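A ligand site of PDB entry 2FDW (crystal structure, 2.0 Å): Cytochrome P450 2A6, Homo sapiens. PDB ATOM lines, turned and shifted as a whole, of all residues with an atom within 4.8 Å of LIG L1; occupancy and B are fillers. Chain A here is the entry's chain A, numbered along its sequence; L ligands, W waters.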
ATOM      1  N   LEU A  69      22.563  -1.506  -6.717  1.00  0.00           N
ATOM      2  CA  LEU A  69      21.638  -1.241  -7.811  1.00  0.00           C
ATOM      3  C   LEU A  69      21.276  -2.429  -8.706  1.00  0.00           C
ATOM      4  O   LEU A  69      20.220  -2.427  -9.351  1.00  0.00           O
ATOM      5  CB  LEU A  69      22.144  -0.060  -8.648  1.00  0.00           C
ATOM      6  CG  LEU A  69      21.812   1.337  -8.098  1.00  0.00           C
ATOM      7  CD1 LEU A  69      22.443   1.562  -6.733  1.00  0.00           C
ATOM      8  CD2 LEU A  69      22.305   2.411  -9.093  1.00  0.00           C
ATOM      9  N   ARG A  79      13.316   6.213  -5.931  1.00  0.00           N
ATOM     10  CA  ARG A  79      13.880   7.451  -6.467  1.00  0.00           C
ATOM     11  C   ARG A  79      14.110   8.445  -5.322  1.00  0.00           C
ATOM     12  O   ARG A  79      13.185   8.741  -4.558  1.00  0.00           O
ATOM     13  CB  ARG A  79      12.945   8.066  -7.506  1.00  0.00           C
ATOM     14  CG  ARG A  79      13.333   9.486  -7.974  1.00  0.00           C
ATOM     15  CD  ARG A  79      14.710   9.533  -8.658  1.00  0.00           C
ATOM     16  NE  ARG A  79      14.732   8.897  -9.977  1.00  0.00           N
ATOM     17  CZ  ARG A  79      15.778   8.216 -10.452  1.00  0.00           C
ATOM     18  NH1 ARG A  79      16.874   8.103  -9.716  1.00  0.00           N
ATOM     19  NH2 ARG A  79      15.728   7.657 -11.650  1.00  0.00           N
ATOM     20  N   VAL A  94       7.743  11.151 -14.732  1.00  0.00           N
ATOM     21  CA  VAL A  94       8.359   9.831 -14.681  1.00  0.00           C
ATOM     22  C   VAL A  94       9.692   9.724 -13.936  1.00  0.00           C
ATOM     23  O   VAL A  94       9.954   8.711 -13.279  1.00  0.00           O
ATOM     24  CB  VAL A  94       8.571   9.279 -16.109  1.00  0.00           C
ATOM     25  CG1 VAL A  94       9.540  10.170 -16.877  1.00  0.00           C
ATOM     26  CG2 VAL A  94       9.085   7.842 -16.048  1.00  0.00           C
ATOM     27  N   VAL A  95      10.524  10.753 -14.028  1.00  0.00           N
ATOM     28  CA  VAL A  95      11.838  10.727 -13.379  1.00  0.00           C
ATOM     29  C   VAL A  95      11.838  10.822 -11.861  1.00  0.00           C
ATOM     30  O   VAL A  95      12.318   9.930 -11.168  1.00  0.00           O
ATOM     31  CB  VAL A  95      12.757  11.877 -13.910  1.00  0.00           C
ATOM     32  CG1 VAL A  95      14.104  11.827 -13.186  1.00  0.00           C
ATOM     33  CG2 VAL A  95      12.960  11.754 -15.404  1.00  0.00           C
ATOM     34  N   ARG A 106       6.664   5.161 -16.314  1.00  0.00           N
ATOM     35  CA  ARG A 106       7.833   4.599 -16.997  1.00  0.00           C
ATOM     36  C   ARG A 106       7.446   3.555 -18.039  1.00  0.00           C
ATOM     37  O   ARG A 106       8.006   3.513 -19.139  1.00  0.00           O
ATOM     38  CB  ARG A 106       8.816   3.984 -15.994  1.00  0.00           C
ATOM     39  CG  ARG A 106       9.980   3.249 -16.654  1.00  0.00           C
ATOM     40  CD  ARG A 106      11.093   2.887 -15.668  1.00  0.00           C
ATOM     41  NE  ARG A 106      12.108   2.035 -16.283  1.00  0.00           N
ATOM     42  CZ  ARG A 106      13.420   2.281 -16.266  1.00  0.00           C
ATOM     43  NH1 ARG A 106      13.885   3.370 -15.655  1.00  0.00           N
ATOM     44  NH2 ARG A 106      14.262   1.453 -16.862  1.00  0.00           N
ATOM     45  N   LEU A 113       7.690   5.727 -26.509  1.00  0.00           N
ATOM     46  CA  LEU A 113       8.946   6.130 -27.148  1.00  0.00           C
ATOM     47  C   LEU A 113       9.246   5.160 -28.315  1.00  0.00           C
ATOM     48  O   LEU A 113       9.660   5.584 -29.402  1.00  0.00           O
ATOM     49  CB  LEU A 113      10.077   6.097 -26.118  1.00  0.00           C
ATOM     50  CG  LEU A 113      10.941   7.348 -25.892  1.00  0.00           C
ATOM     51  CD1 LEU A 113      10.097   8.608 -25.857  1.00  0.00           C
ATOM     52  CD2 LEU A 113      11.703   7.167 -24.572  1.00  0.00           C
ATOM     53  N   ILE A 160      14.576  14.601 -29.696  1.00  0.00           N
ATOM     54  CA  ILE A 160      13.528  14.316 -28.721  1.00  0.00           C
ATOM     55  C   ILE A 160      12.323  15.243 -28.945  1.00  0.00           C
ATOM     56  O   ILE A 160      11.185  14.863 -28.678  1.00  0.00           O
ATOM     57  CB  ILE A 160      14.052  14.439 -27.270  1.00  0.00           C
ATOM     58  CG1 ILE A 160      13.000  13.898 -26.302  1.00  0.00           C
ATOM     59  CG2 ILE A 160      14.417  15.889 -26.941  1.00  0.00           C
ATOM     60  CD1 ILE A 160      12.792  12.390 -26.389  1.00  0.00           C
ATOM     61  N   LEU A 276      11.510  14.321 -20.428  1.00  0.00           N
ATOM     62  CA  LEU A 276      12.099  13.873 -21.691  1.00  0.00           C
ATOM     63  C   LEU A 276      12.757  15.010 -22.450  1.00  0.00           C
ATOM     64  O   LEU A 276      13.839  14.840 -23.028  1.00  0.00           O
ATOM     65  CB  LEU A 276      11.034  13.200 -22.566  1.00  0.00           C
ATOM     66  CG  LEU A 276      10.346  11.974 -21.960  1.00  0.00           C
ATOM     67  CD1 LEU A 276       9.227  11.506 -22.877  1.00  0.00           C
ATOM     68  CD2 LEU A 276      11.369  10.865 -21.732  1.00  0.00           C
ATOM     69  N   GLY A 279      15.885  15.984 -19.979  1.00  0.00           N
ATOM     70  CA  GLY A 279      16.751  14.825 -19.886  1.00  0.00           C
ATOM     71  C   GLY A 279      17.305  14.370 -21.229  1.00  0.00           C
ATOM     72  O   GLY A 279      18.461  13.947 -21.317  1.00  0.00           O
ATOM     73  N   GLY A 280      16.490  14.458 -22.266  1.00  0.00           N
ATOM     74  CA  GLY A 280      16.930  14.033 -23.577  1.00  0.00           C
ATOM     75  C   GLY A 280      17.718  15.064 -24.359  1.00  0.00           C
ATOM     76  O   GLY A 280      18.163  14.795 -25.477  1.00  0.00           O
ATOM     77  N   THR A 283      21.912  16.316 -21.491  1.00  0.00           N
ATOM     78  CA  THR A 283      22.858  15.241 -21.225  1.00  0.00           C
ATOM     79  C   THR A 283      23.705  14.957 -22.465  1.00  0.00           C
ATOM     80  O   THR A 283      24.923  14.985 -22.412  1.00  0.00           O
ATOM     81  CB  THR A 283      22.142  13.941 -20.791  1.00  0.00           C
ATOM     82  OG1 THR A 283      21.116  13.600 -21.743  1.00  0.00           O
ATOM     83  CG2 THR A 283      21.512  14.108 -19.433  1.00  0.00           C
ATOM     84  N   VAL A 284      23.027  14.678 -23.572  1.00  0.00           N
ATOM     85  CA  VAL A 284      23.722  14.394 -24.819  1.00  0.00           C
ATOM     86  C   VAL A 284      24.492  15.622 -25.316  1.00  0.00           C
ATOM     87  O   VAL A 284      25.637  15.491 -25.777  1.00  0.00           O
ATOM     88  CB  VAL A 284      22.728  13.942 -25.900  1.00  0.00           C
ATOM     89  CG1 VAL A 284      23.457  13.660 -27.208  1.00  0.00           C
ATOM     90  CG2 VAL A 284      22.007  12.685 -25.419  1.00  0.00           C
ATOM     91  N   THR A 287      27.696  15.924 -23.452  1.00  0.00           N
ATOM     92  CA  THR A 287      28.642  14.883 -23.855  1.00  0.00           C
ATOM     93  C   THR A 287      29.324  15.249 -25.187  1.00  0.00           C
ATOM     94  O   THR A 287      30.538  15.083 -25.353  1.00  0.00           O
ATOM     95  CB  THR A 287      27.933  13.508 -24.000  1.00  0.00           C
ATOM     96  OG1 THR A 287      27.313  13.153 -22.761  1.00  0.00           O
ATOM     97  CG2 THR A 287      28.943  12.414 -24.394  1.00  0.00           C
ATOM     98  N   GLN A 338      32.379   9.413 -22.690  1.00  0.00           N
ATOM     99  CA  GLN A 338      31.363   9.334 -21.658  1.00  0.00           C
ATOM    100  C   GLN A 338      31.969   8.997 -20.299  1.00  0.00           C
ATOM    101  O   GLN A 338      31.496   9.486 -19.277  1.00  0.00           O
ATOM    102  CB  GLN A 338      30.312   8.285 -22.025  1.00  0.00           C
ATOM    103  CG  GLN A 338      29.429   8.675 -23.186  1.00  0.00           C
ATOM    104  CD  GLN A 338      28.135   7.882 -23.212  1.00  0.00           C
ATOM    105  OE1 GLN A 338      28.064   6.794 -23.794  1.00  0.00           O
ATOM    106  NE2 GLN A 338      27.097   8.406 -22.556  1.00  0.00           N
ATOM    107  N   VAL A 343      29.299  12.954 -17.097  1.00  0.00           N
ATOM    108  CA  VAL A 343      28.245  13.976 -17.130  1.00  0.00           C
ATOM    109  C   VAL A 343      27.305  14.086 -15.927  1.00  0.00           C
ATOM    110  O   VAL A 343      26.954  15.190 -15.503  1.00  0.00           O
ATOM    111  CB  VAL A 343      27.425  13.838 -18.433  1.00  0.00           C
ATOM    112  CG1 VAL A 343      26.339  14.916 -18.494  1.00  0.00           C
ATOM    113  CG2 VAL A 343      28.352  13.971 -19.637  1.00  0.00           C
ATOM    114  N   ILE A 344      26.885  12.942 -15.387  1.00  0.00           N
ATOM    115  CA  ILE A 344      26.007  12.930 -14.205  1.00  0.00           C
ATOM    116  C   ILE A 344      26.844  12.154 -13.202  1.00  0.00           C
ATOM    117  O   ILE A 344      26.596  10.970 -12.944  1.00  0.00           O
ATOM    118  CB  ILE A 344      24.691  12.174 -14.485  1.00  0.00           C
ATOM    119  CG1 ILE A 344      24.036  12.713 -15.765  1.00  0.00           C
ATOM    120  CG2 ILE A 344      23.737  12.316 -13.294  1.00  0.00           C
ATOM    121  CD1 ILE A 344      23.707  14.217 -15.712  1.00  0.00           C
ATOM    122  N   SER A 347      24.892  10.355 -10.449  1.00  0.00           N
ATOM    123  CA  SER A 347      23.618   9.832 -10.936  1.00  0.00           C
ATOM    124  C   SER A 347      22.482  10.693 -10.401  1.00  0.00           C
ATOM    125  O   SER A 347      22.675  11.852 -10.055  1.00  0.00           O
ATOM    126  CB  SER A 347      23.456   8.386 -10.444  1.00  0.00           C
ATOM    127  OG  SER A 347      22.371   7.728 -11.064  1.00  0.00           O
ATOM    128  N   LEU A 348      21.280  10.133 -10.397  1.00  0.00           N
ATOM    129  CA  LEU A 348      20.120  10.800  -9.818  1.00  0.00           C
ATOM    130  C   LEU A 348      19.886   9.919  -8.589  1.00  0.00           C
ATOM    131  O   LEU A 348      19.908   8.698  -8.692  1.00  0.00           O
ATOM    132  CB  LEU A 348      18.908  10.741 -10.760  1.00  0.00           C
ATOM    133  CG  LEU A 348      18.858  11.821 -11.855  1.00  0.00           C
ATOM    134  CD1 LEU A 348      20.053  11.687 -12.774  1.00  0.00           C
ATOM    135  CD2 LEU A 348      17.581  11.661 -12.662  1.00  0.00           C
ATOM    136  N   ARG A 350      18.854   7.562  -5.523  1.00  0.00           N
ATOM    137  CA  ARG A 350      17.971   6.412  -5.400  1.00  0.00           C
ATOM    138  C   ARG A 350      17.541   6.464  -3.942  1.00  0.00           C
ATOM    139  O   ARG A 350      17.939   7.368  -3.215  1.00  0.00           O
ATOM    140  CB  ARG A 350      18.713   5.081  -5.625  1.00  0.00           C
ATOM    141  CG  ARG A 350      19.091   4.765  -7.068  1.00  0.00           C
ATOM    142  CD  ARG A 350      17.850   4.594  -7.926  1.00  0.00           C
ATOM    143  NE  ARG A 350      18.173   4.105  -9.270  1.00  0.00           N
ATOM    144  CZ  ARG A 350      18.301   2.817  -9.576  1.00  0.00           C
ATOM    145  NH1 ARG A 350      18.120   1.893  -8.634  1.00  0.00           N
ATOM    146  NH2 ARG A 350      18.582   2.451 -10.814  1.00  0.00           N
ATOM    147  N   LEU A 373      28.497   7.312  -9.603  1.00  0.00           N
ATOM    148  CA  LEU A 373      28.835   6.851 -10.948  1.00  0.00           C
ATOM    149  C   LEU A 373      30.250   7.240 -11.351  1.00  0.00           C
ATOM    150  O   LEU A 373      30.978   6.433 -11.925  1.00  0.00           O
ATOM    151  CB  LEU A 373      27.836   7.400 -11.976  1.00  0.00           C
ATOM    152  CG  LEU A 373      26.364   7.022 -11.801  1.00  0.00           C
ATOM    153  CD1 LEU A 373      25.604   7.421 -13.063  1.00  0.00           C
ATOM    154  CD2 LEU A 373      26.220   5.523 -11.546  1.00  0.00           C
ATOM    155  N   PRO A 409      27.680   5.207 -17.236  1.00  0.00           N
ATOM    156  CA  PRO A 409      27.268   6.611 -17.336  1.00  0.00           C
ATOM    157  C   PRO A 409      25.762   6.800 -17.319  1.00  0.00           C
ATOM    158  O   PRO A 409      25.258   7.871 -16.982  1.00  0.00           O
ATOM    159  CB  PRO A 409      27.894   7.056 -18.660  1.00  0.00           C
ATOM    160  CG  PRO A 409      27.832   5.808 -19.484  1.00  0.00           C
ATOM    161  CD  PRO A 409      28.283   4.742 -18.496  1.00  0.00           C
ATOM    162  N   PHE A 410      25.038   5.749 -17.706  1.00  0.00           N
ATOM    163  CA  PHE A 410      23.581   5.760 -17.731  1.00  0.00           C
ATOM    164  C   PHE A 410      23.068   5.060 -16.476  1.00  0.00           C
ATOM    165  O   PHE A 410      21.873   4.768 -16.352  1.00  0.00           O
ATOM    166  CB  PHE A 410      23.059   5.008 -18.958  1.00  0.00           C
ATOM    167  CG  PHE A 410      23.489   5.581 -20.272  1.00  0.00           C
ATOM    168  CD1 PHE A 410      22.843   6.675 -20.826  1.00  0.00           C
ATOM    169  CD2 PHE A 410      24.543   5.000 -20.993  1.00  0.00           C
ATOM    170  CE1 PHE A 410      23.216   7.185 -22.072  1.00  0.00           C
ATOM    171  CE2 PHE A 410      24.921   5.497 -22.239  1.00  0.00           C
ATOM    172  CZ  PHE A 410      24.259   6.594 -22.777  1.00  0.00           C
ATOM    173  N   SER A 411      23.980   4.800 -15.538  1.00  0.00           N
ATOM    174  CA  SER A 411      23.645   4.109 -14.307  1.00  0.00           C
ATOM    175  C   SER A 411      23.168   2.688 -14.645  1.00  0.00           C
ATOM    176  O   SER A 411      23.221   2.276 -15.808  1.00  0.00           O
ATOM    177  CB  SER A 411      22.551   4.849 -13.531  1.00  0.00           C
ATOM    178  OG  SER A 411      22.296   4.230 -12.281  1.00  0.00           O
ATOM    179  N   ILE A 412      22.705   1.968 -13.632  1.00  0.00           N
ATOM    180  CA  ILE A 412      22.227   0.604 -13.813  1.00  0.00           C
ATOM    181  C   ILE A 412      21.085   0.317 -12.843  1.00  0.00           C
ATOM    182  O   ILE A 412      20.819   1.097 -11.933  1.00  0.00           O
ATOM    183  CB  ILE A 412      23.374  -0.395 -13.566  1.00  0.00           C
ATOM    184  CG1 ILE A 412      24.043  -0.091 -12.220  1.00  0.00           C
ATOM    185  CG2 ILE A 412      24.402  -0.293 -14.700  1.00  0.00           C
ATOM    186  CD1 ILE A 412      25.333  -0.861 -11.966  1.00  0.00           C
ATOM    187  N   ARG A 415      15.776   1.633 -12.194  1.00  0.00           N
ATOM    188  CA  ARG A 415      15.390   2.994 -12.537  1.00  0.00           C
ATOM    189  C   ARG A 415      16.479   3.617 -13.416  1.00  0.00           C
ATOM    190  O   ARG A 415      16.661   4.829 -13.437  1.00  0.00           O
ATOM    191  CB  ARG A 415      15.183   3.841 -11.281  1.00  0.00           C
ATOM    192  CG  ARG A 415      13.979   3.433 -10.425  1.00  0.00           C
ATOM    193  CD  ARG A 415      12.659   3.702 -11.126  1.00  0.00           C
ATOM    194  NE  ARG A 415      12.425   5.125 -11.369  1.00  0.00           N
ATOM    195  CZ  ARG A 415      11.771   5.941 -10.547  1.00  0.00           C
ATOM    196  NH1 ARG A 415      11.629   7.222 -10.865  1.00  0.00           N
ATOM    197  NH2 ARG A 415      11.241   5.487  -9.412  1.00  0.00           N
ATOM    198  N   ASN A 416      17.186   2.768 -14.166  1.00  0.00           N
ATOM    199  CA  ASN A 416      18.252   3.211 -15.052  1.00  0.00           C
ATOM    200  C   ASN A 416      17.697   4.050 -16.193  1.00  0.00           C
ATOM    201  O   ASN A 416      16.487   4.063 -16.444  1.00  0.00           O
ATOM    202  CB  ASN A 416      19.011   1.989 -15.604  1.00  0.00           C
ATOM    203  CG  ASN A 416      18.209   1.229 -16.653  1.00  0.00           C
ATOM    204  OD1 ASN A 416      16.984   1.142 -16.573  1.00  0.00           O
ATOM    205  ND2 ASN A 416      18.903   0.653 -17.628  1.00  0.00           N
ATOM    206  N   CYS A 417      18.580   4.749 -16.908  1.00  0.00           N
ATOM    207  CA  CYS A 417      18.178   5.604 -18.019  1.00  0.00           C
ATOM    208  C   CYS A 417      17.503   4.848 -19.156  1.00  0.00           C
ATOM    209  O   CYS A 417      18.157   4.058 -19.834  1.00  0.00           O
ATOM    210  CB  CYS A 417      19.391   6.353 -18.584  1.00  0.00           C
ATOM    211  SG  CYS A 417      18.995   7.549 -19.871  1.00  0.00           S
ATOM    212  N   PHE A 418      16.212   5.073 -19.395  1.00  0.00           N
ATOM    213  CA  PHE A 418      15.590   4.365 -20.505  1.00  0.00           C
ATOM    214  C   PHE A 418      15.759   5.156 -21.792  1.00  0.00           C
ATOM    215  O   PHE A 418      15.238   4.783 -22.847  1.00  0.00           O
ATOM    216  CB  PHE A 418      14.125   3.986 -20.219  1.00  0.00           C
ATOM    217  CG  PHE A 418      13.192   5.141 -19.918  1.00  0.00           C
ATOM    218  CD1 PHE A 418      12.684   5.917 -20.949  1.00  0.00           C
ATOM    219  CD2 PHE A 418      12.714   5.329 -18.626  1.00  0.00           C
ATOM    220  CE1 PHE A 418      11.678   6.881 -20.698  1.00  0.00           C
ATOM    221  CE2 PHE A 418      11.713   6.288 -18.363  1.00  0.00           C
ATOM    222  CZ  PHE A 418      11.193   7.059 -19.400  1.00  0.00           C
ATOM    223  N   GLY A 419      16.525   6.242 -21.710  1.00  0.00           N
ATOM    224  CA  GLY A 419      16.813   7.039 -22.883  1.00  0.00           C
ATOM    225  C   GLY A 419      18.178   6.622 -23.428  1.00  0.00           C
ATOM    226  O   GLY A 419      18.693   7.204 -24.392  1.00  0.00           O
ATOM    227  N   LEU A 422      18.439   5.762 -27.321  1.00  0.00           N
ATOM    228  CA  LEU A 422      18.394   6.949 -28.164  1.00  0.00           C
ATOM    229  C   LEU A 422      19.704   7.714 -28.026  1.00  0.00           C
ATOM    230  O   LEU A 422      20.336   8.073 -29.021  1.00  0.00           O
ATOM    231  CB  LEU A 422      17.224   7.855 -27.736  1.00  0.00           C
ATOM    232  CG  LEU A 422      17.042   9.153 -28.524  1.00  0.00           C
ATOM    233  CD1 LEU A 422      16.636   8.838 -29.960  1.00  0.00           C
ATOM    234  CD2 LEU A 422      15.976  10.011 -27.853  1.00  0.00           C
ATOM    235  N   ALA A 423      20.123   7.944 -26.790  1.00  0.00           N
ATOM    236  CA  ALA A 423      21.362   8.659 -26.523  1.00  0.00           C
ATOM    237  C   ALA A 423      22.549   8.078 -27.288  1.00  0.00           C
ATOM    238  O   ALA A 423      23.300   8.810 -27.912  1.00  0.00           O
ATOM    239  CB  ALA A 423      21.650   8.636 -25.031  1.00  0.00           C
ATOM    240  N   LEU A 427      24.729   9.847 -30.126  1.00  0.00           N
ATOM    241  CA  LEU A 427      26.150  10.053 -29.939  1.00  0.00           C
ATOM    242  C   LEU A 427      26.952   9.494 -31.096  1.00  0.00           C
ATOM    243  O   LEU A 427      27.843  10.157 -31.617  1.00  0.00           O
ATOM    244  CB  LEU A 427      26.615   9.405 -28.618  1.00  0.00           C
ATOM    245  CG  LEU A 427      26.152  10.098 -27.341  1.00  0.00           C
ATOM    246  CD1 LEU A 427      26.681   9.342 -26.136  1.00  0.00           C
ATOM    247  CD2 LEU A 427      26.654  11.541 -27.316  1.00  0.00           C
HETATM  248  C1  LIG L   1      17.631   8.780 -15.951  1.00  0.00           C
HETATM  249  C2  LIG L   1      21.987   9.575 -17.677  1.00  0.00           C
HETATM  250  C3  LIG L   1      20.135  10.465 -21.942  1.00  0.00           C
HETATM  251  C4  LIG L   1      15.794  10.029 -20.116  1.00  0.00           C
HETATM  252  C5  LIG L   1      19.023   8.730 -16.043  1.00  0.00           C
HETATM  253  C6  LIG L   1      19.922   8.476 -14.990  1.00  0.00           C
HETATM  254  C7  LIG L   1      21.186   8.789 -15.485  1.00  0.00           C
HETATM  255  C8  LIG L   1      20.983   9.220 -16.800  1.00  0.00           C
HETATM  256  C9  LIG L   1      22.568   8.692 -14.729  1.00  0.00           C
HETATM  257  C10 LIG L   1      19.555   7.935 -13.604  1.00  0.00           C
HETATM  258  C11 LIG L   1      19.565   6.431 -13.526  1.00  0.00           C
HETATM  259  C12 LIG L   1      19.244   5.822 -12.172  1.00  0.00           C
HETATM  260  O1  LIG L   1      19.790   4.784 -11.859  1.00  0.00           O
HETATM  261  O2  LIG L   1      18.463   6.348 -11.401  1.00  0.00           O
HETATM  262  C13 LIG L   1      21.949   9.942 -19.019  1.00  0.00           C
HETATM  263  C14 LIG L   1      23.063  10.224 -19.849  1.00  0.00           C
HETATM  264  C15 LIG L   1      22.500  10.465 -21.135  1.00  0.00           C
HETATM  265  C16 LIG L   1      21.098  10.313 -20.950  1.00  0.00           C
HETATM  266  C17 LIG L   1      24.509  10.230 -19.392  1.00  0.00           C
HETATM  267  C18 LIG L   1      23.145  10.799 -22.377  1.00  0.00           C
HETATM  268  C19 LIG L   1      24.568  10.727 -22.795  1.00  0.00           C
HETATM  269  C20 LIG L   1      18.746  10.358 -21.898  1.00  0.00           C
HETATM  270  C21 LIG L   1      17.895  10.628 -22.962  1.00  0.00           C
HETATM  271  C22 LIG L   1      16.594  10.595 -22.441  1.00  0.00           C
HETATM  272  C23 LIG L   1      16.766  10.304 -21.059  1.00  0.00           C
HETATM  273  C24 LIG L   1      18.309  10.906 -24.445  1.00  0.00           C
HETATM  274  C25 LIG L   1      15.358  10.799 -23.007  1.00  0.00           C
HETATM  275  C26 LIG L   1      14.712  10.122 -24.070  1.00  0.00           C
HETATM  276  C27 LIG L   1      15.891   9.546 -18.850  1.00  0.00           C
HETATM  277  C28 LIG L   1      14.803   9.334 -17.991  1.00  0.00           C
HETATM  278  C29 LIG L   1      15.311   8.959 -16.785  1.00  0.00           C
HETATM  279  C30 LIG L   1      16.702   8.988 -16.955  1.00  0.00           C
HETATM  280  C31 LIG L   1      13.319   9.475 -18.350  1.00  0.00           C
HETATM  281  C32 LIG L   1      14.543   8.600 -15.465  1.00  0.00           C
HETATM  282  C33 LIG L   1      14.227   7.067 -15.382  1.00  0.00           C
HETATM  283  C34 LIG L   1      13.471   6.539 -14.119  1.00  0.00           C
HETATM  284  O3  LIG L   1      12.919   5.476 -14.134  1.00  0.00           O
HETATM  285  O4  LIG L   1      13.450   7.212 -13.089  1.00  0.00           O
HETATM  286  N1  LIG L   1      19.706   9.185 -17.137  1.00  0.00           N
HETATM  287  N2  LIG L   1      20.808  10.004 -19.703  1.00  0.00           N
HETATM  288  N3  LIG L   1      18.080  10.170 -20.779  1.00  0.00           N
HETATM  289  N4  LIG L   1      17.003   9.339 -18.205  1.00  0.00           N
HETATM  290 FE1  LIG L   1      18.904   9.644 -18.974  1.00  0.00          FE
HETATM  291  C1  LG2 L   2      16.483  17.295 -15.266  1.00  0.00           C
HETATM  292  C2  LG2 L   2      15.248  17.971 -15.074  1.00  0.00           C
HETATM  293  C3  LG2 L   2      14.045  17.288 -15.430  1.00  0.00           C
HETATM  294  N1  LG2 L   2      14.031  16.013 -15.956  1.00  0.00           N
HETATM  295  C4  LG2 L   2      15.224  15.376 -16.138  1.00  0.00           C
HETATM  296  C5  LG2 L   2      16.494  15.968 -15.808  1.00  0.00           C
HETATM  297  C6  LG2 L   2      17.730  15.255 -16.025  1.00  0.00           C
HETATM  298  C7  LG2 L   2      19.062  15.581 -15.807  1.00  0.00           C
HETATM  299  C8  LG2 L   2      19.844  14.446 -16.222  1.00  0.00           C
HETATM  300  C9  LG2 L   2      18.951  13.493 -16.656  1.00  0.00           C
HETATM  301  O1  LG2 L   2      17.646  13.963 -16.548  1.00  0.00           O
HETATM  302  C10 LG2 L   2      19.091  12.121 -17.195  1.00  0.00           C
HETATM  303  N2  LG2 L   2      18.552  11.862 -18.504  1.00  0.00           N
HETATM  304  O   HOH W   1      10.279   5.795 -13.553  1.00  0.00           O
HETATM  305  O   HOH W   2      21.070   6.010  -9.622  1.00  0.00           O
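The guanidinium group of Arg 79 lies within hydrogen-bond range of the backbone carbonyl oxygen of Leu 348 (3.3 Å).
O of Val 95 sits at hydrogen-bond distance from NH1 of Arg 415, at 2.8 Å.
The side-chain sulfur of Cys 417 sits close to the backbone NH of Gly 419 (3.3 Å).
The guanidinium group of Arg 79 lies within hydrogen-bond range of the backbone carbonyl oxygen of Val 95, 2.9 Å away.
N of Cys 417 sits at hydrogen-bond distance from O of Phe 410, at 3.3 Å.
OD1 of Asn 416 lies within hydrogen-bond range of NH2 of Arg 106 (2.8 Å).
The backbone carbonyl oxygen (O) of Gly 279 sits at hydrogen-bond distance from the side-chain hydroxyl (OG1) of Thr 283, at 2.7 Å.
O of Arg 415 is in hydrogen-bond range of NH2 of Arg 79 (3.5 Å).
A nitrogen (N2) of LG2 L2 is bound to an iron atom (FE1) of LIG L1 (2.3 Å).
Water W1 lies within hydrogen-bond range of O3 of LIG L1, O of Val 94 and NE of Arg 415.
Water W2 lies within hydrogen-bond range of the side-chain hydroxyl of Ser 347, an oxygen (O1) of LIG L1, the backbone carbonyl oxygen of Leu 348, the side-chain hydroxyl of Ser 411 and the guanidinium group of Arg 350.
NH2 of Arg 79 lies within salt-bridge range of O4 of LIG L1 (2.7 Å).
The guanidinium group (NE) of Arg 415 is in salt-bridge range of an oxygen (O3) of LIG L1, at 2.8 Å.
An oxygen (O1) of LIG L1 lies within salt-bridge range of the guanidinium group (NH2) of Arg 350 (2.8 Å).
FE1 of LIG L1 is bound by SG of Cys 417.
O3 of LIG L1 lies within salt-bridge range of NH1 of Arg 106.
The side-chain hydroxyl (OG) of Ser 411 lies within hydrogen-bond range of an oxygen (O1) of LIG L1 (2.6 Å).
Val 94 touches LIG L1.
O of Val 95 touches O4 of LIG L1, 3.5 Å away.
CD1 of Ile 160 touches C26 of LIG L1 (3.8 Å).
O of Gly 279 touches C20 of LIG L1, at 3.6 Å.
Gly 280 touches LIG L1.
Thr 283 touches LIG L1.
Val 284 touches LIG L1.
Thr 287 touches LIG L1.
Gln 338 touches LIG L1 (NE2 to C19, 3.4 Å).
Ser 347 touches LIG L1 (OG to C9, 3.8 Å).
O of Leu 348 touches O2 of LIG L1, 3.9 Å away.
Leu 373 touches LIG L1 (CD1 to C9, 3.7 Å).
Pro 409 touches LIG L1 (O to C17, 3.5 Å).
CE1 of Phe 410 touches C15 of LIG L1, at 3.5 Å.
Ile 412 touches LIG L1.
Asn 416 touches LIG L1.
Phe 418 touches LIG L1.
CA of Gly 419 touches C22 of LIG L1 (3.6 Å).
Leu 422 touches LIG L1.
Ala 423 touches LIG L1.
26 residues have an atom within 4 Å of LIG L1: Arg 79, Val 94, Val 95, Arg 106, Ile 160, Gly 279, Gly 280, Thr 283, Val 284, Thr 287, Gln 338, Ser 347, Leu 348, Arg 350, Leu 373, Pro 409, Phe 410, Ser 411, Ile 412, Arg 415, Asn 416, Cys 417, Phe 418, Gly 419, Leu 422 and Ala 423.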
